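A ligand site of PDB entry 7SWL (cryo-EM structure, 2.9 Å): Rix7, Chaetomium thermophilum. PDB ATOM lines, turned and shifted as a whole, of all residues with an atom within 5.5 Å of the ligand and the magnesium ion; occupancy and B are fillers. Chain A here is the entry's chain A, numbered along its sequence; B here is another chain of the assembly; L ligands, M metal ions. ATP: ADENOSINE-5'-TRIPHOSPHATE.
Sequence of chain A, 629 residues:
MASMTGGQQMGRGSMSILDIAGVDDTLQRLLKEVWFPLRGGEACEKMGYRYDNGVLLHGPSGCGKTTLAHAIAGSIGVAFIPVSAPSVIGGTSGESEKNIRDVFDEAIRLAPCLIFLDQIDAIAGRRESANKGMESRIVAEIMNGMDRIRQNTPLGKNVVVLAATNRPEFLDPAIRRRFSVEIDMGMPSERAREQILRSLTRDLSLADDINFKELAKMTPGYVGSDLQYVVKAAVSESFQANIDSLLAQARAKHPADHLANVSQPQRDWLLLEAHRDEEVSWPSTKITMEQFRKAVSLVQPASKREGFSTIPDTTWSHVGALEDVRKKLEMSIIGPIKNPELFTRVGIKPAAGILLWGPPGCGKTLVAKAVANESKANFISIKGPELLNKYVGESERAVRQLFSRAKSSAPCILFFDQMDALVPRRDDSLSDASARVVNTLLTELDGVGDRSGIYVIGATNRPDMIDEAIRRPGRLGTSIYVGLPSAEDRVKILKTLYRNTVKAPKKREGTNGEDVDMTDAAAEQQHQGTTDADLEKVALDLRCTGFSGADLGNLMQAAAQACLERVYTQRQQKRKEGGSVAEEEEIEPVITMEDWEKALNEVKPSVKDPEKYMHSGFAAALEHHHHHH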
ATOM      1  N   HIS A 318      36.918 -17.166  -4.720  1.00  0.00           N
ATOM      2  CA  HIS A 318      35.589 -17.535  -5.181  1.00  0.00           C
ATOM      3  C   HIS A 318      34.652 -17.899  -4.042  1.00  0.00           C
ATOM      4  O   HIS A 318      33.439 -17.978  -4.268  1.00  0.00           O
ATOM      5  CB  HIS A 318      35.664 -18.698  -6.159  1.00  0.00           C
ATOM      6  CG  HIS A 318      36.327 -18.359  -7.467  1.00  0.00           C
ATOM      7  ND1 HIS A 318      37.664 -18.049  -7.560  1.00  0.00           N
ATOM      8  CD2 HIS A 318      35.828 -18.279  -8.715  1.00  0.00           C
ATOM      9  CE1 HIS A 318      37.970 -17.795  -8.817  1.00  0.00           C
ATOM     10  NE2 HIS A 318      36.874 -17.927  -9.542  1.00  0.00           N
ATOM     11  N   VAL A 319      35.172 -18.133  -2.841  1.00  0.00           N
ATOM     12  CA  VAL A 319      34.371 -18.489  -1.687  1.00  0.00           C
ATOM     13  C   VAL A 319      34.155 -17.248  -0.850  1.00  0.00           C
ATOM     14  O   VAL A 319      35.118 -16.662  -0.330  1.00  0.00           O
ATOM     15  CB  VAL A 319      35.051 -19.605  -0.862  1.00  0.00           C
ATOM     16  CG1 VAL A 319      34.190 -19.955   0.346  1.00  0.00           C
ATOM     17  CG2 VAL A 319      35.300 -20.831  -1.715  1.00  0.00           C
ATOM     18  N   GLY A 320      32.893 -16.839  -0.710  1.00  0.00           N
ATOM     19  CA  GLY A 320      32.538 -15.675   0.089  1.00  0.00           C
ATOM     20  C   GLY A 320      32.094 -16.100   1.472  1.00  0.00           C
ATOM     21  O   GLY A 320      31.316 -17.037   1.626  1.00  0.00           O
ATOM     22  N   ALA A 321      32.607 -15.395   2.481  1.00  0.00           N
ATOM     23  CA  ALA A 321      32.309 -15.658   3.893  1.00  0.00           C
ATOM     24  C   ALA A 321      32.713 -17.099   4.198  1.00  0.00           C
ATOM     25  O   ALA A 321      33.763 -17.553   3.704  1.00  0.00           O
ATOM     26  CB  ALA A 321      30.862 -15.324   4.177  1.00  0.00           C
ATOM     27  N   LEU A 322      31.932 -17.839   4.994  1.00  0.00           N
ATOM     28  CA  LEU A 322      32.278 -19.189   5.410  1.00  0.00           C
ATOM     29  C   LEU A 322      33.652 -19.242   6.070  1.00  0.00           C
ATOM     30  O   LEU A 322      34.440 -20.157   5.847  1.00  0.00           O
ATOM     31  CB  LEU A 322      32.208 -20.180   4.240  1.00  0.00           C
ATOM     32  CG  LEU A 322      30.825 -20.509   3.679  1.00  0.00           C
ATOM     33  CD1 LEU A 322      30.943 -21.349   2.418  1.00  0.00           C
ATOM     34  CD2 LEU A 322      29.998 -21.241   4.733  1.00  0.00           C
ATOM     35  N   GLY A 358      24.709 -29.902   4.988  1.00  0.00           N
ATOM     36  CA  GLY A 358      23.903 -28.718   5.124  1.00  0.00           C
ATOM     37  C   GLY A 358      22.839 -28.632   4.048  1.00  0.00           C
ATOM     38  O   GLY A 358      22.687 -29.543   3.226  1.00  0.00           O
ATOM     39  N   PRO A 359      22.082 -27.542   4.028  1.00  0.00           N
ATOM     40  CA  PRO A 359      21.062 -27.376   2.991  1.00  0.00           C
ATOM     41  C   PRO A 359      21.710 -27.196   1.632  1.00  0.00           C
ATOM     42  O   PRO A 359      22.858 -26.737   1.531  1.00  0.00           O
ATOM     43  CB  PRO A 359      20.316 -26.097   3.436  1.00  0.00           C
ATOM     44  CG  PRO A 359      21.244 -25.393   4.337  1.00  0.00           C
ATOM     45  CD  PRO A 359      22.048 -26.450   5.028  1.00  0.00           C
ATOM     46  N   PRO A 360      21.006 -27.566   0.562  1.00  0.00           N
ATOM     47  CA  PRO A 360      21.592 -27.442  -0.778  1.00  0.00           C
ATOM     48  C   PRO A 360      21.807 -25.997  -1.186  1.00  0.00           C
ATOM     49  O   PRO A 360      21.063 -25.094  -0.809  1.00  0.00           O
ATOM     50  CB  PRO A 360      20.561 -28.132  -1.681  1.00  0.00           C
ATOM     51  CG  PRO A 360      19.286 -28.048  -0.928  1.00  0.00           C
ATOM     52  CD  PRO A 360      19.663 -28.149   0.517  1.00  0.00           C
ATOM     53  N   GLY A 361      22.849 -25.788  -2.002  1.00  0.00           N
ATOM     54  CA  GLY A 361      23.162 -24.472  -2.523  1.00  0.00           C
ATOM     55  C   GLY A 361      23.950 -23.574  -1.608  1.00  0.00           C
ATOM     56  O   GLY A 361      24.051 -22.377  -1.886  1.00  0.00           O
ATOM     57  N   CYS A 362      24.540 -24.112  -0.543  1.00  0.00           N
ATOM     58  CA  CYS A 362      25.209 -23.298   0.468  1.00  0.00           C
ATOM     59  C   CYS A 362      26.720 -23.353   0.399  1.00  0.00           C
ATOM     60  O   CYS A 362      27.378 -22.604   1.130  1.00  0.00           O
ATOM     61  CB  CYS A 362      24.738 -23.701   1.865  1.00  0.00           C
ATOM     62  SG  CYS A 362      23.027 -23.252   2.201  1.00  0.00           S
ATOM     63  N   GLY A 363      27.300 -24.202  -0.440  1.00  0.00           N
ATOM     64  CA  GLY A 363      28.731 -24.137  -0.687  1.00  0.00           C
ATOM     65  C   GLY A 363      29.547 -25.329  -0.243  1.00  0.00           C
ATOM     66  O   GLY A 363      30.755 -25.207  -0.060  1.00  0.00           O
ATOM     67  N   LYS A 364      28.905 -26.491  -0.063  1.00  0.00           N
ATOM     68  CA  LYS A 364      29.653 -27.684   0.313  1.00  0.00           C
ATOM     69  C   LYS A 364      30.606 -28.107  -0.797  1.00  0.00           C
ATOM     70  O   LYS A 364      31.763 -28.457  -0.533  1.00  0.00           O
ATOM     71  CB  LYS A 364      28.697 -28.822   0.658  1.00  0.00           C
ATOM     72  CG  LYS A 364      27.752 -28.508   1.783  1.00  0.00           C
ATOM     73  CD  LYS A 364      26.874 -29.694   2.096  1.00  0.00           C
ATOM     74  CE  LYS A 364      25.884 -29.958   0.977  1.00  0.00           C
ATOM     75  NZ  LYS A 364      24.946 -28.831   0.814  1.00  0.00           N
ATOM     76  N   THR A 365      30.142 -28.109  -2.048  1.00  0.00           N
ATOM     77  CA  THR A 365      31.004 -28.443  -3.165  1.00  0.00           C
ATOM     78  C   THR A 365      31.965 -27.309  -3.502  1.00  0.00           C
ATOM     79  O   THR A 365      33.079 -27.556  -3.973  1.00  0.00           O
ATOM     80  CB  THR A 365      30.161 -28.806  -4.393  1.00  0.00           C
ATOM     81  OG1 THR A 365      29.263 -29.870  -4.058  1.00  0.00           O
ATOM     82  CG2 THR A 365      31.040 -29.252  -5.551  1.00  0.00           C
ATOM     83  N   LEU A 366      31.557 -26.059  -3.251  1.00  0.00           N
ATOM     84  CA  LEU A 366      32.413 -24.927  -3.558  1.00  0.00           C
ATOM     85  C   LEU A 366      33.672 -24.940  -2.707  1.00  0.00           C
ATOM     86  O   LEU A 366      34.782 -24.760  -3.214  1.00  0.00           O
ATOM     87  CB  LEU A 366      31.642 -23.619  -3.361  1.00  0.00           C
ATOM     88  CG  LEU A 366      32.368 -22.335  -3.725  1.00  0.00           C
ATOM     89  CD1 LEU A 366      32.582 -22.249  -5.224  1.00  0.00           C
ATOM     90  CD2 LEU A 366      31.592 -21.130  -3.237  1.00  0.00           C
ATOM     91  N   VAL A 367      33.527 -25.153  -1.401  1.00  0.00           N
ATOM     92  CA  VAL A 367      34.694 -25.143  -0.519  1.00  0.00           C
ATOM     93  C   VAL A 367      35.560 -26.380  -0.752  1.00  0.00           C
ATOM     94  O   VAL A 367      36.784 -26.313  -0.612  1.00  0.00           O
ATOM     95  CB  VAL A 367      34.263 -25.018   0.951  1.00  0.00           C
ATOM     96  CG1 VAL A 367      33.496 -23.728   1.164  1.00  0.00           C
ATOM     97  CG2 VAL A 367      33.451 -26.210   1.394  1.00  0.00           C
ATOM     98  N   ASP A 417      31.253 -36.651  -3.540  1.00  0.00           N
ATOM     99  CA  ASP A 417      30.145 -35.723  -3.668  1.00  0.00           C
ATOM    100  C   ASP A 417      28.825 -36.488  -3.683  1.00  0.00           C
ATOM    101  O   ASP A 417      28.708 -37.518  -4.347  1.00  0.00           O
ATOM    102  CB  ASP A 417      30.290 -34.895  -4.953  1.00  0.00           C
ATOM    103  CG  ASP A 417      29.532 -33.590  -4.878  1.00  0.00           C
ATOM    104  OD1 ASP A 417      29.059 -33.237  -3.783  1.00  0.00           O
ATOM    105  OD2 ASP A 417      29.419 -32.920  -5.929  1.00  0.00           O
ATOM    106  N   GLN A 418      27.849 -35.961  -2.945  1.00  0.00           N
ATOM    107  CA  GLN A 418      26.571 -36.635  -2.740  1.00  0.00           C
ATOM    108  C   GLN A 418      26.791 -38.035  -2.186  1.00  0.00           C
ATOM    109  O   GLN A 418      26.374 -39.044  -2.759  1.00  0.00           O
ATOM    110  CB  GLN A 418      25.735 -36.672  -4.025  1.00  0.00           C
ATOM    111  CG  GLN A 418      25.683 -35.363  -4.786  1.00  0.00           C
ATOM    112  CD  GLN A 418      24.872 -34.298  -4.078  1.00  0.00           C
ATOM    113  OE1 GLN A 418      24.262 -34.544  -3.045  1.00  0.00           O
ATOM    114  NE2 GLN A 418      24.866 -33.100  -4.648  1.00  0.00           N
ATOM    115  N   ALA A 459      30.483 -34.905   1.022  1.00  0.00           N
ATOM    116  CA  ALA A 459      29.465 -33.876   0.999  1.00  0.00           C
ATOM    117  C   ALA A 459      28.104 -34.516   0.745  1.00  0.00           C
ATOM    118  O   ALA A 459      27.973 -35.371  -0.133  1.00  0.00           O
ATOM    119  CB  ALA A 459      29.759 -32.806  -0.054  1.00  0.00           C
ATOM    120  N   THR A 460      27.111 -34.085   1.508  1.00  0.00           N
ATOM    121  CA  THR A 460      25.741 -34.562   1.333  1.00  0.00           C
ATOM    122  C   THR A 460      24.800 -33.554   1.967  1.00  0.00           C
ATOM    123  O   THR A 460      25.115 -32.953   2.991  1.00  0.00           O
ATOM    124  CB  THR A 460      25.536 -35.954   1.956  1.00  0.00           C
ATOM    125  OG1 THR A 460      24.164 -36.328   1.846  1.00  0.00           O
ATOM    126  CG2 THR A 460      25.937 -35.949   3.425  1.00  0.00           C
ATOM    127  N   ASN A 461      23.648 -33.355   1.329  1.00  0.00           N
ATOM    128  CA  ASN A 461      22.642 -32.438   1.846  1.00  0.00           C
ATOM    129  C   ASN A 461      21.516 -33.145   2.578  1.00  0.00           C
ATOM    130  O   ASN A 461      20.602 -32.484   3.075  1.00  0.00           O
ATOM    131  CB  ASN A 461      22.067 -31.584   0.703  1.00  0.00           C
ATOM    132  CG  ASN A 461      21.691 -32.411  -0.505  1.00  0.00           C
ATOM    133  OD1 ASN A 461      22.312 -33.428  -0.795  1.00  0.00           O
ATOM    134  ND2 ASN A 461      20.665 -31.981  -1.213  1.00  0.00           N
ATOM    135  N   ILE A 493      28.959 -12.670   0.296  1.00  0.00           N
ATOM    136  CA  ILE A 493      28.753 -13.591  -0.820  1.00  0.00           C
ATOM    137  C   ILE A 493      28.348 -12.840  -2.076  1.00  0.00           C
ATOM    138  O   ILE A 493      28.833 -13.135  -3.169  1.00  0.00           O
ATOM    139  CB  ILE A 493      27.716 -14.662  -0.434  1.00  0.00           C
ATOM    140  CG1 ILE A 493      28.222 -15.465   0.761  1.00  0.00           C
ATOM    141  CG2 ILE A 493      27.424 -15.567  -1.614  1.00  0.00           C
ATOM    142  CD1 ILE A 493      27.336 -16.632   1.124  1.00  0.00           C
ATOM    143  N   THR A 496      31.320 -11.145  -3.478  1.00  0.00           N
ATOM    144  CA  THR A 496      32.208 -12.116  -4.114  1.00  0.00           C
ATOM    145  C   THR A 496      31.711 -12.506  -5.491  1.00  0.00           C
ATOM    146  O   THR A 496      32.498 -12.573  -6.445  1.00  0.00           O
ATOM    147  CB  THR A 496      32.316 -13.355  -3.224  1.00  0.00           C
ATOM    148  OG1 THR A 496      32.882 -12.999  -1.956  1.00  0.00           O
ATOM    149  CG2 THR A 496      33.201 -14.404  -3.887  1.00  0.00           C
ATOM    150  N   LEU A 497      30.410 -12.756  -5.637  1.00  0.00           N
ATOM    151  CA  LEU A 497      29.866 -13.180  -6.920  1.00  0.00           C
ATOM    152  C   LEU A 497      29.945 -12.060  -7.952  1.00  0.00           C
ATOM    153  O   LEU A 497      30.346 -12.300  -9.095  1.00  0.00           O
ATOM    154  CB  LEU A 497      28.423 -13.645  -6.742  1.00  0.00           C
ATOM    155  CG  LEU A 497      28.205 -14.916  -5.914  1.00  0.00           C
ATOM    156  CD1 LEU A 497      26.719 -15.167  -5.727  1.00  0.00           C
ATOM    157  CD2 LEU A 497      28.867 -16.104  -6.571  1.00  0.00           C
ATOM    158  N   GLY A 549      23.656 -19.327  -1.073  1.00  0.00           N
ATOM    159  CA  GLY A 549      24.648 -18.846  -2.017  1.00  0.00           C
ATOM    160  C   GLY A 549      24.176 -18.951  -3.453  1.00  0.00           C
ATOM    161  O   GLY A 549      24.423 -18.047  -4.262  1.00  0.00           O
ATOM    162  N   ALA A 550      23.489 -20.041  -3.792  1.00  0.00           N
ATOM    163  CA  ALA A 550      22.967 -20.194  -5.151  1.00  0.00           C
ATOM    164  C   ALA A 550      21.881 -19.176  -5.447  1.00  0.00           C
ATOM    165  O   ALA A 550      21.792 -18.677  -6.578  1.00  0.00           O
ATOM    166  CB  ALA A 550      22.438 -21.613  -5.342  1.00  0.00           C
ATOM    167  N   ASP B 446      25.082 -29.938 -11.289  1.00  0.00           N
ATOM    168  CA  ASP B 446      25.939 -28.998 -10.566  1.00  0.00           C
ATOM    169  C   ASP B 446      26.839 -29.817  -9.635  1.00  0.00           C
ATOM    170  O   ASP B 446      26.401 -30.259  -8.575  1.00  0.00           O
ATOM    171  CB  ASP B 446      25.120 -27.979  -9.795  1.00  0.00           C
ATOM    172  CG  ASP B 446      25.939 -26.795  -9.344  1.00  0.00           C
ATOM    173  OD1 ASP B 446      27.163 -26.788  -9.578  1.00  0.00           O
ATOM    174  OD2 ASP B 446      25.359 -25.857  -8.747  1.00  0.00           O
ATOM    175  N   ALA B 469      16.610 -30.724  -3.826  1.00  0.00           N
ATOM    176  CA  ALA B 469      17.958 -30.384  -4.265  1.00  0.00           C
ATOM    177  C   ALA B 469      18.020 -30.106  -5.755  1.00  0.00           C
ATOM    178  O   ALA B 469      18.807 -29.268  -6.203  1.00  0.00           O
ATOM    179  CB  ALA B 469      18.932 -31.506  -3.899  1.00  0.00           C
ATOM    180  N   ARG B 472      16.999 -26.134  -7.382  1.00  0.00           N
ATOM    181  CA  ARG B 472      17.791 -25.059  -6.816  1.00  0.00           C
ATOM    182  C   ARG B 472      18.576 -24.390  -7.941  1.00  0.00           C
ATOM    183  O   ARG B 472      18.871 -25.036  -8.955  1.00  0.00           O
ATOM    184  CB  ARG B 472      18.756 -25.557  -5.730  1.00  0.00           C
ATOM    185  CG  ARG B 472      20.035 -26.203  -6.248  1.00  0.00           C
ATOM    186  CD  ARG B 472      21.131 -26.104  -5.210  1.00  0.00           C
ATOM    187  NE  ARG B 472      22.366 -26.729  -5.653  1.00  0.00           N
ATOM    188  CZ  ARG B 472      23.299 -26.129  -6.362  1.00  0.00           C
ATOM    189  NH1 ARG B 472      23.173 -24.872  -6.756  1.00  0.00           N
ATOM    190  NH2 ARG B 472      24.389 -26.801  -6.702  1.00  0.00           N
ATOM    191  N   PRO B 473      18.894 -23.107  -7.789  1.00  0.00           N
ATOM    192  CA  PRO B 473      19.685 -22.420  -8.836  1.00  0.00           C
ATOM    193  C   PRO B 473      21.015 -23.127  -9.058  1.00  0.00           C
ATOM    194  O   PRO B 473      21.818 -23.277  -8.136  1.00  0.00           O
ATOM    195  CB  PRO B 473      19.860 -21.018  -8.256  1.00  0.00           C
ATOM    196  CG  PRO B 473      18.685 -20.839  -7.382  1.00  0.00           C
ATOM    197  CD  PRO B 473      18.426 -22.170  -6.764  1.00  0.00           C
ATOM    198  N   ARG B 475      20.834 -26.247 -10.923  1.00  0.00           N
ATOM    199  CA  ARG B 475      20.320 -27.460 -11.535  1.00  0.00           C
ATOM    200  C   ARG B 475      19.023 -27.205 -12.295  1.00  0.00           C
ATOM    201  O   ARG B 475      18.971 -27.395 -13.511  1.00  0.00           O
ATOM    202  CB  ARG B 475      20.108 -28.526 -10.459  1.00  0.00           C
ATOM    203  CG  ARG B 475      21.324 -28.767  -9.603  1.00  0.00           C
ATOM    204  CD  ARG B 475      21.188 -30.041  -8.806  1.00  0.00           C
ATOM    205  NE  ARG B 475      22.444 -30.415  -8.164  1.00  0.00           N
ATOM    206  CZ  ARG B 475      22.720 -30.201  -6.885  1.00  0.00           C
ATOM    207  NH1 ARG B 475      21.839 -29.623  -6.077  1.00  0.00           N
ATOM    208  NH2 ARG B 475      23.897 -30.577  -6.406  1.00  0.00           N
HETATM  209  PG  ATP L   1      24.178 -29.358  -3.045  1.00  0.00           P
HETATM  210  O1G ATP L   1      23.926 -29.949  -1.687  1.00  0.00           O
HETATM  211  O2G ATP L   1      25.235 -30.087  -3.824  1.00  0.00           O
HETATM  212  O3G ATP L   1      22.915 -29.160  -3.836  1.00  0.00           O
HETATM  213  PB  ATP L   1      26.220 -27.373  -2.351  1.00  0.00           P
HETATM  214  O1B ATP L   1      27.216 -28.223  -3.048  1.00  0.00           O
HETATM  215  O2B ATP L   1      26.269 -27.269  -0.876  1.00  0.00           O
HETATM  216  O3B ATP L   1      24.756 -27.864  -2.782  1.00  0.00           O
HETATM  217  PA  ATP L   1      27.307 -25.410  -4.161  1.00  0.00           P
HETATM  218  O1A ATP L   1      27.116 -26.296  -5.337  1.00  0.00           O
HETATM  219  O2A ATP L   1      28.701 -25.227  -3.687  1.00  0.00           O
HETATM  220  O3A ATP L   1      26.362 -25.891  -2.973  1.00  0.00           O
HETATM  221  O5' ATP L   1      26.732 -23.941  -4.495  1.00  0.00           O
HETATM  222  C5' ATP L   1      26.319 -23.632  -5.825  1.00  0.00           C
HETATM  223  C4' ATP L   1      26.805 -22.268  -6.216  1.00  0.00           C
HETATM  224  O4' ATP L   1      26.319 -21.288  -5.263  1.00  0.00           O
HETATM  225  C3' ATP L   1      28.311 -22.066  -6.209  1.00  0.00           C
HETATM  226  O3' ATP L   1      28.937 -22.586  -7.367  1.00  0.00           O
HETATM  227  C2' ATP L   1      28.419 -20.550  -6.082  1.00  0.00           C
HETATM  228  O2' ATP L   1      28.139 -19.946  -7.337  1.00  0.00           O
HETATM  229  C1' ATP L   1      27.259 -20.237  -5.129  1.00  0.00           C
HETATM  230  N9  ATP L   1      27.682 -20.162  -3.723  1.00  0.00           N
HETATM  231  C8  ATP L   1      27.256 -20.938  -2.672  1.00  0.00           C
HETATM  232  N7  ATP L   1      27.810 -20.635  -1.529  1.00  0.00           N
HETATM  233  C5  ATP L   1      28.650 -19.582  -1.843  1.00  0.00           C
HETATM  234  C6  ATP L   1      29.526 -18.806  -1.057  1.00  0.00           C
HETATM  235  N6  ATP L   1      29.694 -18.984   0.258  1.00  0.00           N
HETATM  236  N1  ATP L   1      30.230 -17.830  -1.674  1.00  0.00           N
HETATM  237  C2  ATP L   1      30.062 -17.652  -2.989  1.00  0.00           C
HETATM  238  N3  ATP L   1      29.277 -18.314  -3.829  1.00  0.00           N
HETATM  239  C4  ATP L   1      28.589 -19.274  -3.190  1.00  0.00           C
HETATM  240 MG    MG M   1      27.261 -30.004  -3.965  1.00  0.00          MG
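Residues that only touch the magnesium ion: Asp 417 and Gln 418.
The nearest printed residue that does not touch the magnesium ion is Arg 475 of chain B (4.2 Å).
O1B of the ligand binds the magnesium ion (2.0 Å).
The magnesium ion is bound by OG1 of Thr 365 (2.0 Å).
O2G of the ligand binds the magnesium ion (2.0 Å).
O of Cys 362 lies close to N7 of the ligand.
His 318 touches the ligand (O to C2, 3.6 Å).
Leu 322 touches the ligand.
Pro 360 touches the ligand (CB to O3G, 3.4 Å).
CB of Asn 461 touches O1G of the ligand, at 3.4 Å.
Ile 493 touches the ligand.
Leu 497 touches the ligand.
Gly 549 touches the ligand (CA to C8, 3.4 Å).
OD2 of Asp 446 of chain B touches C5' of the ligand, 3.8 Å away.
Hydrophobic or aromatic side chains that line the ligand: Leu 322, Pro 360, Leu 366, Ile 493, Leu 497 and Ala 550.
Within 4 Å of the ligand: His 318, Gly 320, Leu 322, Pro 360, Gly 361, Cys 362, Gly 363, Lys 364, Thr 365, Leu 366, Gln 418, Asn 461, Ile 493, Leu 497, Gly 549, Ala 550, Asp 446 of chain B, Arg 472 of chain B and Arg 475 of chain B.
Along chain A the residues within 4 Å of the ligand span positions 318 to 550.
O of Gly 320 lies within hydrogen-bond range of N6 of the ligand.
N1 of the ligand sits at hydrogen-bond distance from N of Gly 320 (3.0 Å).
The backbone NH of Leu 366 sits at hydrogen-bond distance from an oxygen (O2A) of the ligand (3.0 Å).
O2B of the ligand sits at hydrogen-bond distance from N of Lys 364 (2.9 Å).
An oxygen (O1B) of the ligand sits close to the backbone NH (N) of Thr 365 (3.1 Å).
NE of Arg 472 of chain B is in salt-bridge range of O3G of the ligand (3.1 Å).
The backbone NH (N) of Gly 361 is in hydrogen-bond range of an oxygen (O3B) of the ligand, at 2.9 Å.
The backbone NH (N) of Ala 550 sits at hydrogen-bond distance from an oxygen (O4') of the ligand, 3.4 Å away.
N of Gly 363 lies within hydrogen-bond range of O3A of the ligand.
NE2 of Gln 418 sits close to O2G of the ligand, at 3.1 Å.
An oxygen (O3G) of the ligand is in salt-bridge range of the guanidinium group (NH1) of Arg 475 of chain B.
The side-chain amino group of Lys 364 is in salt-bridge range of an oxygen (O2B) of the ligand, 2.7 Å away.
NE2 of Gln 418 lies close to NH2 of Arg 475 of chain B.
NH2 of Arg 475 of chain B is in hydrogen-bond range of O of Asp 446 of chain B (3.3 Å).
O of Gly 361 lies within hydrogen-bond range of N of Ala 550 (3.1 Å).
The guanidinium group (NH2) of Arg 472 of chain B lies within salt-bridge range of the side-chain carboxylate (OD2) of Asp 446 of chain B (2.5 Å).
O of Gly 358 sits at hydrogen-bond distance from NZ of Lys 364.
The side-chain amide oxygen (OE1) of Gln 418 sits close to the side-chain amide oxygen (OD1) of Asn 461 (3.2 Å).
OG1 of Thr 365 sits close to OD1 of Asp 417, at 3.4 Å.
SG of Cys 362 lies close to O of Pro 359.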
